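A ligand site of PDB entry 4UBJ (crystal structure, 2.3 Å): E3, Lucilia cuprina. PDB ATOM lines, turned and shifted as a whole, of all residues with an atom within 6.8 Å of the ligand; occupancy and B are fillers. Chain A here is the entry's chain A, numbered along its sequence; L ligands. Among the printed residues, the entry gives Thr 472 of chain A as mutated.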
ATOM      1  N   HIS A 134     -32.432  11.608   2.677  1.00  0.00           N
ATOM      2  CA  HIS A 134     -32.375  11.422   1.233  1.00  0.00           C
ATOM      3  C   HIS A 134     -30.945  11.523   0.705  1.00  0.00           C
ATOM      4  O   HIS A 134     -30.050  12.043   1.387  1.00  0.00           O
ATOM      5  CB  HIS A 134     -33.277  12.450   0.549  1.00  0.00           C
ATOM      6  CG  HIS A 134     -32.759  13.849   0.644  1.00  0.00           C
ATOM      7  ND1 HIS A 134     -31.764  14.337  -0.180  1.00  0.00           N
ATOM      8  CD2 HIS A 134     -33.118  14.871   1.456  1.00  0.00           C
ATOM      9  CE1 HIS A 134     -31.523  15.605   0.130  1.00  0.00           C
ATOM     10  NE2 HIS A 134     -32.325  15.950   1.117  1.00  0.00           N
ATOM     11  N   GLY A 135     -30.743  10.985  -0.495  1.00  0.00           N
ATOM     12  CA  GLY A 135     -29.467  11.045  -1.179  1.00  0.00           C
ATOM     13  C   GLY A 135     -29.516  12.117  -2.227  1.00  0.00           C
ATOM     14  O   GLY A 135     -30.431  12.942  -2.229  1.00  0.00           O
ATOM     15  N   GLY A 136     -28.546  12.093  -3.138  1.00  0.00           N
ATOM     16  CA  GLY A 136     -28.421  13.144  -4.140  1.00  0.00           C
ATOM     17  C   GLY A 136     -27.044  13.809  -4.093  1.00  0.00           C
ATOM     18  O   GLY A 136     -26.912  15.009  -4.327  1.00  0.00           O
ATOM     19  N   GLY A 137     -26.033  12.995  -3.779  1.00  0.00           N
ATOM     20  CA  GLY A 137     -24.650  13.410  -3.773  1.00  0.00           C
ATOM     21  C   GLY A 137     -24.358  14.638  -2.919  1.00  0.00           C
ATOM     22  O   GLY A 137     -23.366  15.313  -3.159  1.00  0.00           O
ATOM     23  N   PHE A 138     -25.229  14.912  -1.941  1.00  0.00           N
ATOM     24  CA  PHE A 138     -25.180  16.145  -1.136  1.00  0.00           C
ATOM     25  C   PHE A 138     -25.403  17.441  -1.949  1.00  0.00           C
ATOM     26  O   PHE A 138     -25.205  18.535  -1.439  1.00  0.00           O
ATOM     27  CB  PHE A 138     -23.842  16.257  -0.391  1.00  0.00           C
ATOM     28  CG  PHE A 138     -23.521  15.060   0.475  1.00  0.00           C
ATOM     29  CD1 PHE A 138     -24.067  14.930   1.739  1.00  0.00           C
ATOM     30  CD2 PHE A 138     -22.653  14.066   0.027  1.00  0.00           C
ATOM     31  CE1 PHE A 138     -23.776  13.835   2.529  1.00  0.00           C
ATOM     32  CE2 PHE A 138     -22.350  12.961   0.809  1.00  0.00           C
ATOM     33  CZ  PHE A 138     -22.913  12.857   2.068  1.00  0.00           C
ATOM     34  N   ILE A 140     -28.324  17.532  -4.452  1.00  0.00           N
ATOM     35  CA  ILE A 140     -29.749  17.583  -4.767  1.00  0.00           C
ATOM     36  C   ILE A 140     -30.534  16.717  -3.790  1.00  0.00           C
ATOM     37  O   ILE A 140     -29.951  15.924  -3.041  1.00  0.00           O
ATOM     38  CB  ILE A 140     -30.078  17.097  -6.195  1.00  0.00           C
ATOM     39  CG1 ILE A 140     -29.691  15.615  -6.346  1.00  0.00           C
ATOM     40  CG2 ILE A 140     -29.424  17.997  -7.254  1.00  0.00           C
ATOM     41  CD1 ILE A 140     -30.072  14.993  -7.675  1.00  0.00           C
ATOM     42  N   GLU A 217     -30.268   6.388   1.453  1.00  0.00           N
ATOM     43  CA  GLU A 217     -29.724   5.783   0.247  1.00  0.00           C
ATOM     44  C   GLU A 217     -28.704   6.721  -0.432  1.00  0.00           C
ATOM     45  O   GLU A 217     -28.883   7.950  -0.447  1.00  0.00           O
ATOM     46  CB  GLU A 217     -30.886   5.414  -0.692  1.00  0.00           C
ATOM     47  CG  GLU A 217     -30.534   4.666  -1.953  1.00  0.00           C
ATOM     48  CD  GLU A 217     -30.270   5.607  -3.112  1.00  0.00           C
ATOM     49  OE1 GLU A 217     -30.723   6.772  -3.032  1.00  0.00           O
ATOM     50  OE2 GLU A 217     -29.613   5.177  -4.089  1.00  0.00           O
ATOM     51  N   SER A 218     -27.633   6.138  -0.953  1.00  0.00           N
ATOM     52  CA  SER A 218     -26.548   6.876  -1.607  1.00  0.00           C
ATOM     53  C   SER A 218     -25.914   7.903  -0.653  1.00  0.00           C
ATOM     54  O   SER A 218     -25.376   7.523   0.378  1.00  0.00           O
ATOM     55  CB  SER A 218     -27.063   7.555  -2.868  1.00  0.00           C
ATOM     56  OG  SER A 218     -25.998   7.879  -3.739  1.00  0.00           O
ATOM     57  N   ALA A 219     -26.009   9.196  -0.978  1.00  0.00           N
ATOM     58  CA  ALA A 219     -25.540  10.246  -0.071  1.00  0.00           C
ATOM     59  C   ALA A 219     -26.273  10.162   1.265  1.00  0.00           C
ATOM     60  O   ALA A 219     -25.723  10.516   2.310  1.00  0.00           O
ATOM     61  CB  ALA A 219     -25.718  11.629  -0.693  1.00  0.00           C
ATOM     62  N   GLY A 220     -27.511   9.684   1.245  1.00  0.00           N
ATOM     63  CA  GLY A 220     -28.283   9.520   2.460  1.00  0.00           C
ATOM     64  C   GLY A 220     -27.724   8.407   3.310  1.00  0.00           C
ATOM     65  O   GLY A 220     -27.771   8.472   4.536  1.00  0.00           O
ATOM     66  N   SER A 244     -26.793   1.294  -0.298  1.00  0.00           N
ATOM     67  CA  SER A 244     -25.909   1.724  -1.390  1.00  0.00           C
ATOM     68  C   SER A 244     -25.038   2.928  -1.000  1.00  0.00           C
ATOM     69  O   SER A 244     -25.075   3.955  -1.666  1.00  0.00           O
ATOM     70  CB  SER A 244     -26.706   2.084  -2.647  1.00  0.00           C
ATOM     71  OG  SER A 244     -27.429   0.992  -3.156  1.00  0.00           O
ATOM     72  N   TRP A 251     -16.667   8.919  -2.973  1.00  0.00           N
ATOM     73  CA  TRP A 251     -17.459  10.128  -3.265  1.00  0.00           C
ATOM     74  C   TRP A 251     -18.075  10.796  -2.030  1.00  0.00           C
ATOM     75  O   TRP A 251     -18.775  11.803  -2.153  1.00  0.00           O
ATOM     76  CB  TRP A 251     -18.586   9.769  -4.240  1.00  0.00           C
ATOM     77  CG  TRP A 251     -19.359   8.548  -3.806  1.00  0.00           C
ATOM     78  CD1 TRP A 251     -19.129   7.246  -4.199  1.00  0.00           C
ATOM     79  CD2 TRP A 251     -20.446   8.507  -2.871  1.00  0.00           C
ATOM     80  NE1 TRP A 251     -20.032   6.408  -3.573  1.00  0.00           N
ATOM     81  CE2 TRP A 251     -20.846   7.153  -2.757  1.00  0.00           C
ATOM     82  CE3 TRP A 251     -21.130   9.477  -2.129  1.00  0.00           C
ATOM     83  CZ2 TRP A 251     -21.886   6.745  -1.909  1.00  0.00           C
ATOM     84  CZ3 TRP A 251     -22.174   9.073  -1.303  1.00  0.00           C
ATOM     85  CH2 TRP A 251     -22.534   7.715  -1.201  1.00  0.00           C
ATOM     86  N   MET A 308     -15.917  13.471  -7.496  1.00  0.00           N
ATOM     87  CA  MET A 308     -17.266  13.553  -8.071  1.00  0.00           C
ATOM     88  C   MET A 308     -17.969  14.880  -7.810  1.00  0.00           C
ATOM     89  O   MET A 308     -18.726  15.381  -8.640  1.00  0.00           O
ATOM     90  CB  MET A 308     -18.114  12.399  -7.545  1.00  0.00           C
ATOM     91  CG  MET A 308     -19.492  12.305  -8.168  1.00  0.00           C
ATOM     92  SD  MET A 308     -20.343  10.768  -7.743  1.00  0.00           S
ATOM     93  CE  MET A 308     -19.453   9.566  -8.740  1.00  0.00           C
ATOM     94  N   PHE A 309     -17.726  15.445  -6.633  1.00  0.00           N
ATOM     95  CA  PHE A 309     -18.405  16.659  -6.201  1.00  0.00           C
ATOM     96  C   PHE A 309     -17.389  17.632  -5.598  1.00  0.00           C
ATOM     97  O   PHE A 309     -16.553  17.230  -4.787  1.00  0.00           O
ATOM     98  CB  PHE A 309     -19.491  16.327  -5.162  1.00  0.00           C
ATOM     99  CG  PHE A 309     -20.489  15.296  -5.628  1.00  0.00           C
ATOM    100  CD1 PHE A 309     -21.406  15.581  -6.632  1.00  0.00           C
ATOM    101  CD2 PHE A 309     -20.536  14.044  -5.025  1.00  0.00           C
ATOM    102  CE1 PHE A 309     -22.326  14.639  -7.063  1.00  0.00           C
ATOM    103  CE2 PHE A 309     -21.471  13.082  -5.439  1.00  0.00           C
ATOM    104  CZ  PHE A 309     -22.361  13.381  -6.459  1.00  0.00           C
ATOM    105  N   PHE A 354     -26.353   2.781 -13.299  1.00  0.00           N
ATOM    106  CA  PHE A 354     -26.674   4.180 -13.162  1.00  0.00           C
ATOM    107  C   PHE A 354     -25.853   5.082 -14.109  1.00  0.00           C
ATOM    108  O   PHE A 354     -26.292   6.157 -14.524  1.00  0.00           O
ATOM    109  CB  PHE A 354     -26.450   4.594 -11.710  1.00  0.00           C
ATOM    110  CG  PHE A 354     -26.881   5.974 -11.406  1.00  0.00           C
ATOM    111  CD1 PHE A 354     -26.000   7.038 -11.540  1.00  0.00           C
ATOM    112  CD2 PHE A 354     -28.184   6.237 -10.987  1.00  0.00           C
ATOM    113  CE1 PHE A 354     -26.404   8.324 -11.266  1.00  0.00           C
ATOM    114  CE2 PHE A 354     -28.586   7.515 -10.701  1.00  0.00           C
ATOM    115  CZ  PHE A 354     -27.694   8.566 -10.853  1.00  0.00           C
ATOM    116  N   PHE A 355     -24.646   4.635 -14.456  1.00  0.00           N
ATOM    117  CA  PHE A 355     -23.728   5.479 -15.208  1.00  0.00           C
ATOM    118  C   PHE A 355     -23.887   5.405 -16.718  1.00  0.00           C
ATOM    119  O   PHE A 355     -23.112   6.008 -17.453  1.00  0.00           O
ATOM    120  CB  PHE A 355     -22.286   5.162 -14.787  1.00  0.00           C
ATOM    121  CG  PHE A 355     -22.012   5.517 -13.364  1.00  0.00           C
ATOM    122  CD1 PHE A 355     -21.635   6.793 -13.024  1.00  0.00           C
ATOM    123  CD2 PHE A 355     -22.192   4.581 -12.357  1.00  0.00           C
ATOM    124  CE1 PHE A 355     -21.421   7.130 -11.707  1.00  0.00           C
ATOM    125  CE2 PHE A 355     -21.975   4.909 -11.037  1.00  0.00           C
ATOM    126  CZ  PHE A 355     -21.589   6.185 -10.708  1.00  0.00           C
ATOM    127  N   TYR A 420     -17.460   2.337  -6.564  1.00  0.00           N
ATOM    128  CA  TYR A 420     -18.290   3.261  -5.822  1.00  0.00           C
ATOM    129  C   TYR A 420     -19.084   2.619  -4.694  1.00  0.00           C
ATOM    130  O   TYR A 420     -19.552   3.326  -3.808  1.00  0.00           O
ATOM    131  CB  TYR A 420     -19.259   3.968  -6.773  1.00  0.00           C
ATOM    132  CG  TYR A 420     -18.569   4.896  -7.749  1.00  0.00           C
ATOM    133  CD1 TYR A 420     -17.951   6.066  -7.294  1.00  0.00           C
ATOM    134  CD2 TYR A 420     -18.534   4.619  -9.107  1.00  0.00           C
ATOM    135  CE1 TYR A 420     -17.299   6.934  -8.170  1.00  0.00           C
ATOM    136  CE2 TYR A 420     -17.892   5.482  -9.991  1.00  0.00           C
ATOM    137  CZ  TYR A 420     -17.269   6.636  -9.522  1.00  0.00           C
ATOM    138  OH  TYR A 420     -16.645   7.502 -10.375  1.00  0.00           O
ATOM    139  N   PHE A 421     -19.247   1.292  -4.705  1.00  0.00           N
ATOM    140  CA  PHE A 421     -20.152   0.720  -3.701  1.00  0.00           C
ATOM    141  C   PHE A 421     -19.678  -0.568  -3.019  1.00  0.00           C
ATOM    142  O   PHE A 421     -19.590  -0.609  -1.796  1.00  0.00           O
ATOM    143  CB  PHE A 421     -21.536   0.497  -4.333  1.00  0.00           C
ATOM    144  CG  PHE A 421     -22.203   1.785  -4.817  1.00  0.00           C
ATOM    145  CD1 PHE A 421     -22.660   2.741  -3.911  1.00  0.00           C
ATOM    146  CD2 PHE A 421     -22.350   2.035  -6.171  1.00  0.00           C
ATOM    147  CE1 PHE A 421     -23.247   3.909  -4.361  1.00  0.00           C
ATOM    148  CE2 PHE A 421     -22.939   3.212  -6.622  1.00  0.00           C
ATOM    149  CZ  PHE A 421     -23.391   4.150  -5.712  1.00  0.00           C
ATOM    150  N   TYR A 457     -35.377   9.337 -10.510  1.00  0.00           N
ATOM    151  CA  TYR A 457     -33.974   9.066 -10.799  1.00  0.00           C
ATOM    152  C   TYR A 457     -33.756   8.298 -12.098  1.00  0.00           C
ATOM    153  O   TYR A 457     -32.706   8.394 -12.715  1.00  0.00           O
ATOM    154  CB  TYR A 457     -33.319   8.285  -9.666  1.00  0.00           C
ATOM    155  CG  TYR A 457     -32.845   9.111  -8.507  1.00  0.00           C
ATOM    156  CD1 TYR A 457     -31.709   9.903  -8.620  1.00  0.00           C
ATOM    157  CD2 TYR A 457     -33.494   9.052  -7.285  1.00  0.00           C
ATOM    158  CE1 TYR A 457     -31.255  10.632  -7.540  1.00  0.00           C
ATOM    159  CE2 TYR A 457     -33.050   9.779  -6.203  1.00  0.00           C
ATOM    160  CZ  TYR A 457     -31.927  10.574  -6.337  1.00  0.00           C
ATOM    161  OH  TYR A 457     -31.492  11.299  -5.254  1.00  0.00           O
ATOM    162  N   MET A 460     -33.118  10.535 -14.955  1.00  0.00           N
ATOM    163  CA  MET A 460     -31.817  11.209 -14.925  1.00  0.00           C
ATOM    164  C   MET A 460     -30.697  10.304 -15.431  1.00  0.00           C
ATOM    165  O   MET A 460     -29.852  10.744 -16.213  1.00  0.00           O
ATOM    166  CB  MET A 460     -31.529  11.694 -13.505  1.00  0.00           C
ATOM    167  CG  MET A 460     -30.123  12.216 -13.289  1.00  0.00           C
ATOM    168  SD  MET A 460     -29.642  12.159 -11.540  1.00  0.00           S
ATOM    169  CE  MET A 460     -30.966  13.096 -10.781  1.00  0.00           C
ATOM    170  N   HIS A 471     -28.588   1.405  -9.328  1.00  0.00           N
ATOM    171  CA  HIS A 471     -28.570   2.287  -8.186  1.00  0.00           C
ATOM    172  C   HIS A 471     -29.854   3.147  -8.205  1.00  0.00           C
ATOM    173  O   HIS A 471     -30.176   3.713  -9.244  1.00  0.00           O
ATOM    174  CB  HIS A 471     -27.286   3.136  -8.250  1.00  0.00           C
ATOM    175  CG  HIS A 471     -27.091   4.027  -7.069  1.00  0.00           C
ATOM    176  ND1 HIS A 471     -26.842   3.540  -5.798  1.00  0.00           N
ATOM    177  CD2 HIS A 471     -27.116   5.375  -6.959  1.00  0.00           C
ATOM    178  CE1 HIS A 471     -26.713   4.556  -4.964  1.00  0.00           C
ATOM    179  NE2 HIS A 471     -26.884   5.674  -5.644  1.00  0.00           N
ATOM    180  N   THR A 472     -30.585   3.184  -7.074  1.00  0.00           N
ATOM    181  CA  THR A 472     -31.880   3.890  -6.838  1.00  0.00           C
ATOM    182  C   THR A 472     -33.148   3.202  -7.320  1.00  0.00           C
ATOM    183  O   THR A 472     -34.256   3.730  -7.133  1.00  0.00           O
ATOM    184  CB  THR A 472     -31.954   5.306  -7.473  1.00  0.00           C
ATOM    185  OG1 THR A 472     -32.104   5.190  -8.901  1.00  0.00           O
ATOM    186  CG2 THR A 472     -30.740   6.183  -7.117  1.00  0.00           C
HETATM  187  O1  LIG L   1     -26.404  10.310  -3.522  1.00  0.00           O
HETATM  188  P1  LIG L   1     -25.917   9.214  -4.426  1.00  0.00           P
HETATM  189  O2  LIG L   1     -24.347   9.564  -4.798  1.00  0.00           O
HETATM  190  C1  LIG L   1     -23.440   8.518  -4.739  1.00  0.00           C
HETATM  191  C2  LIG L   1     -22.628   8.550  -6.017  1.00  0.00           C
HETATM  192  O3  LIG L   1     -26.677   9.444  -5.870  1.00  0.00           O
HETATM  193  C3  LIG L   1     -27.979   9.024  -5.983  1.00  0.00           C
HETATM  194  C4  LIG L   1     -28.260   8.737  -7.422  1.00  0.00           C
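Gly 135 touches the ligand. Trp 251 touches the ligand (CD2 to C1, 3.5 Å). SD of Met 308 touches C2 of the ligand (3.6 Å). Phe 354 touches the ligand (CZ to C4, 3.5 Å). Tyr 457 touches the ligand. His 471 touches the ligand (NE2 to C3, 3.5 Å). Thr 472 touches the ligand (CG2 to C4, 3.6 Å). Hydrophobic or aromatic side chains within 4 Å of the ligand: Ala 219, Trp 251, Met 308, Phe 354, Tyr 457 and His 471. Of the 22 residues printed, 11 come within 4 Å of the ligand.
The side-chain hydroxyl of Ser 218 sits at hydrogen-bond distance from a ring nitrogen (NE2) of His 471, 3.0 Å away. N of Ser 218 lies close to O of Ser 244 (3.4 Å). The indole nitrogen (NE1) of Trp 251 lies within hydrogen-bond range of the backbone carbonyl oxygen (O) of Tyr 420 (3.1 Å). The side-chain carboxylate (OE2) of Glu 217 lies close to a ring nitrogen (NE2) of His 471, 3.2 Å away.
The side-chain hydroxyl (OG) of Ser 218 is covalently linked to a phosphorus (P1) of the ligand (1.5 Å). The backbone NH (N) of Gly 137 is in hydrogen-bond range of an oxygen (O1) of the ligand (2.7 Å). N of Ala 219 sits at hydrogen-bond distance from O1 of the ligand. N of Gly 136 sits at hydrogen-bond distance from O1 of the ligand, at 2.8 Å.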
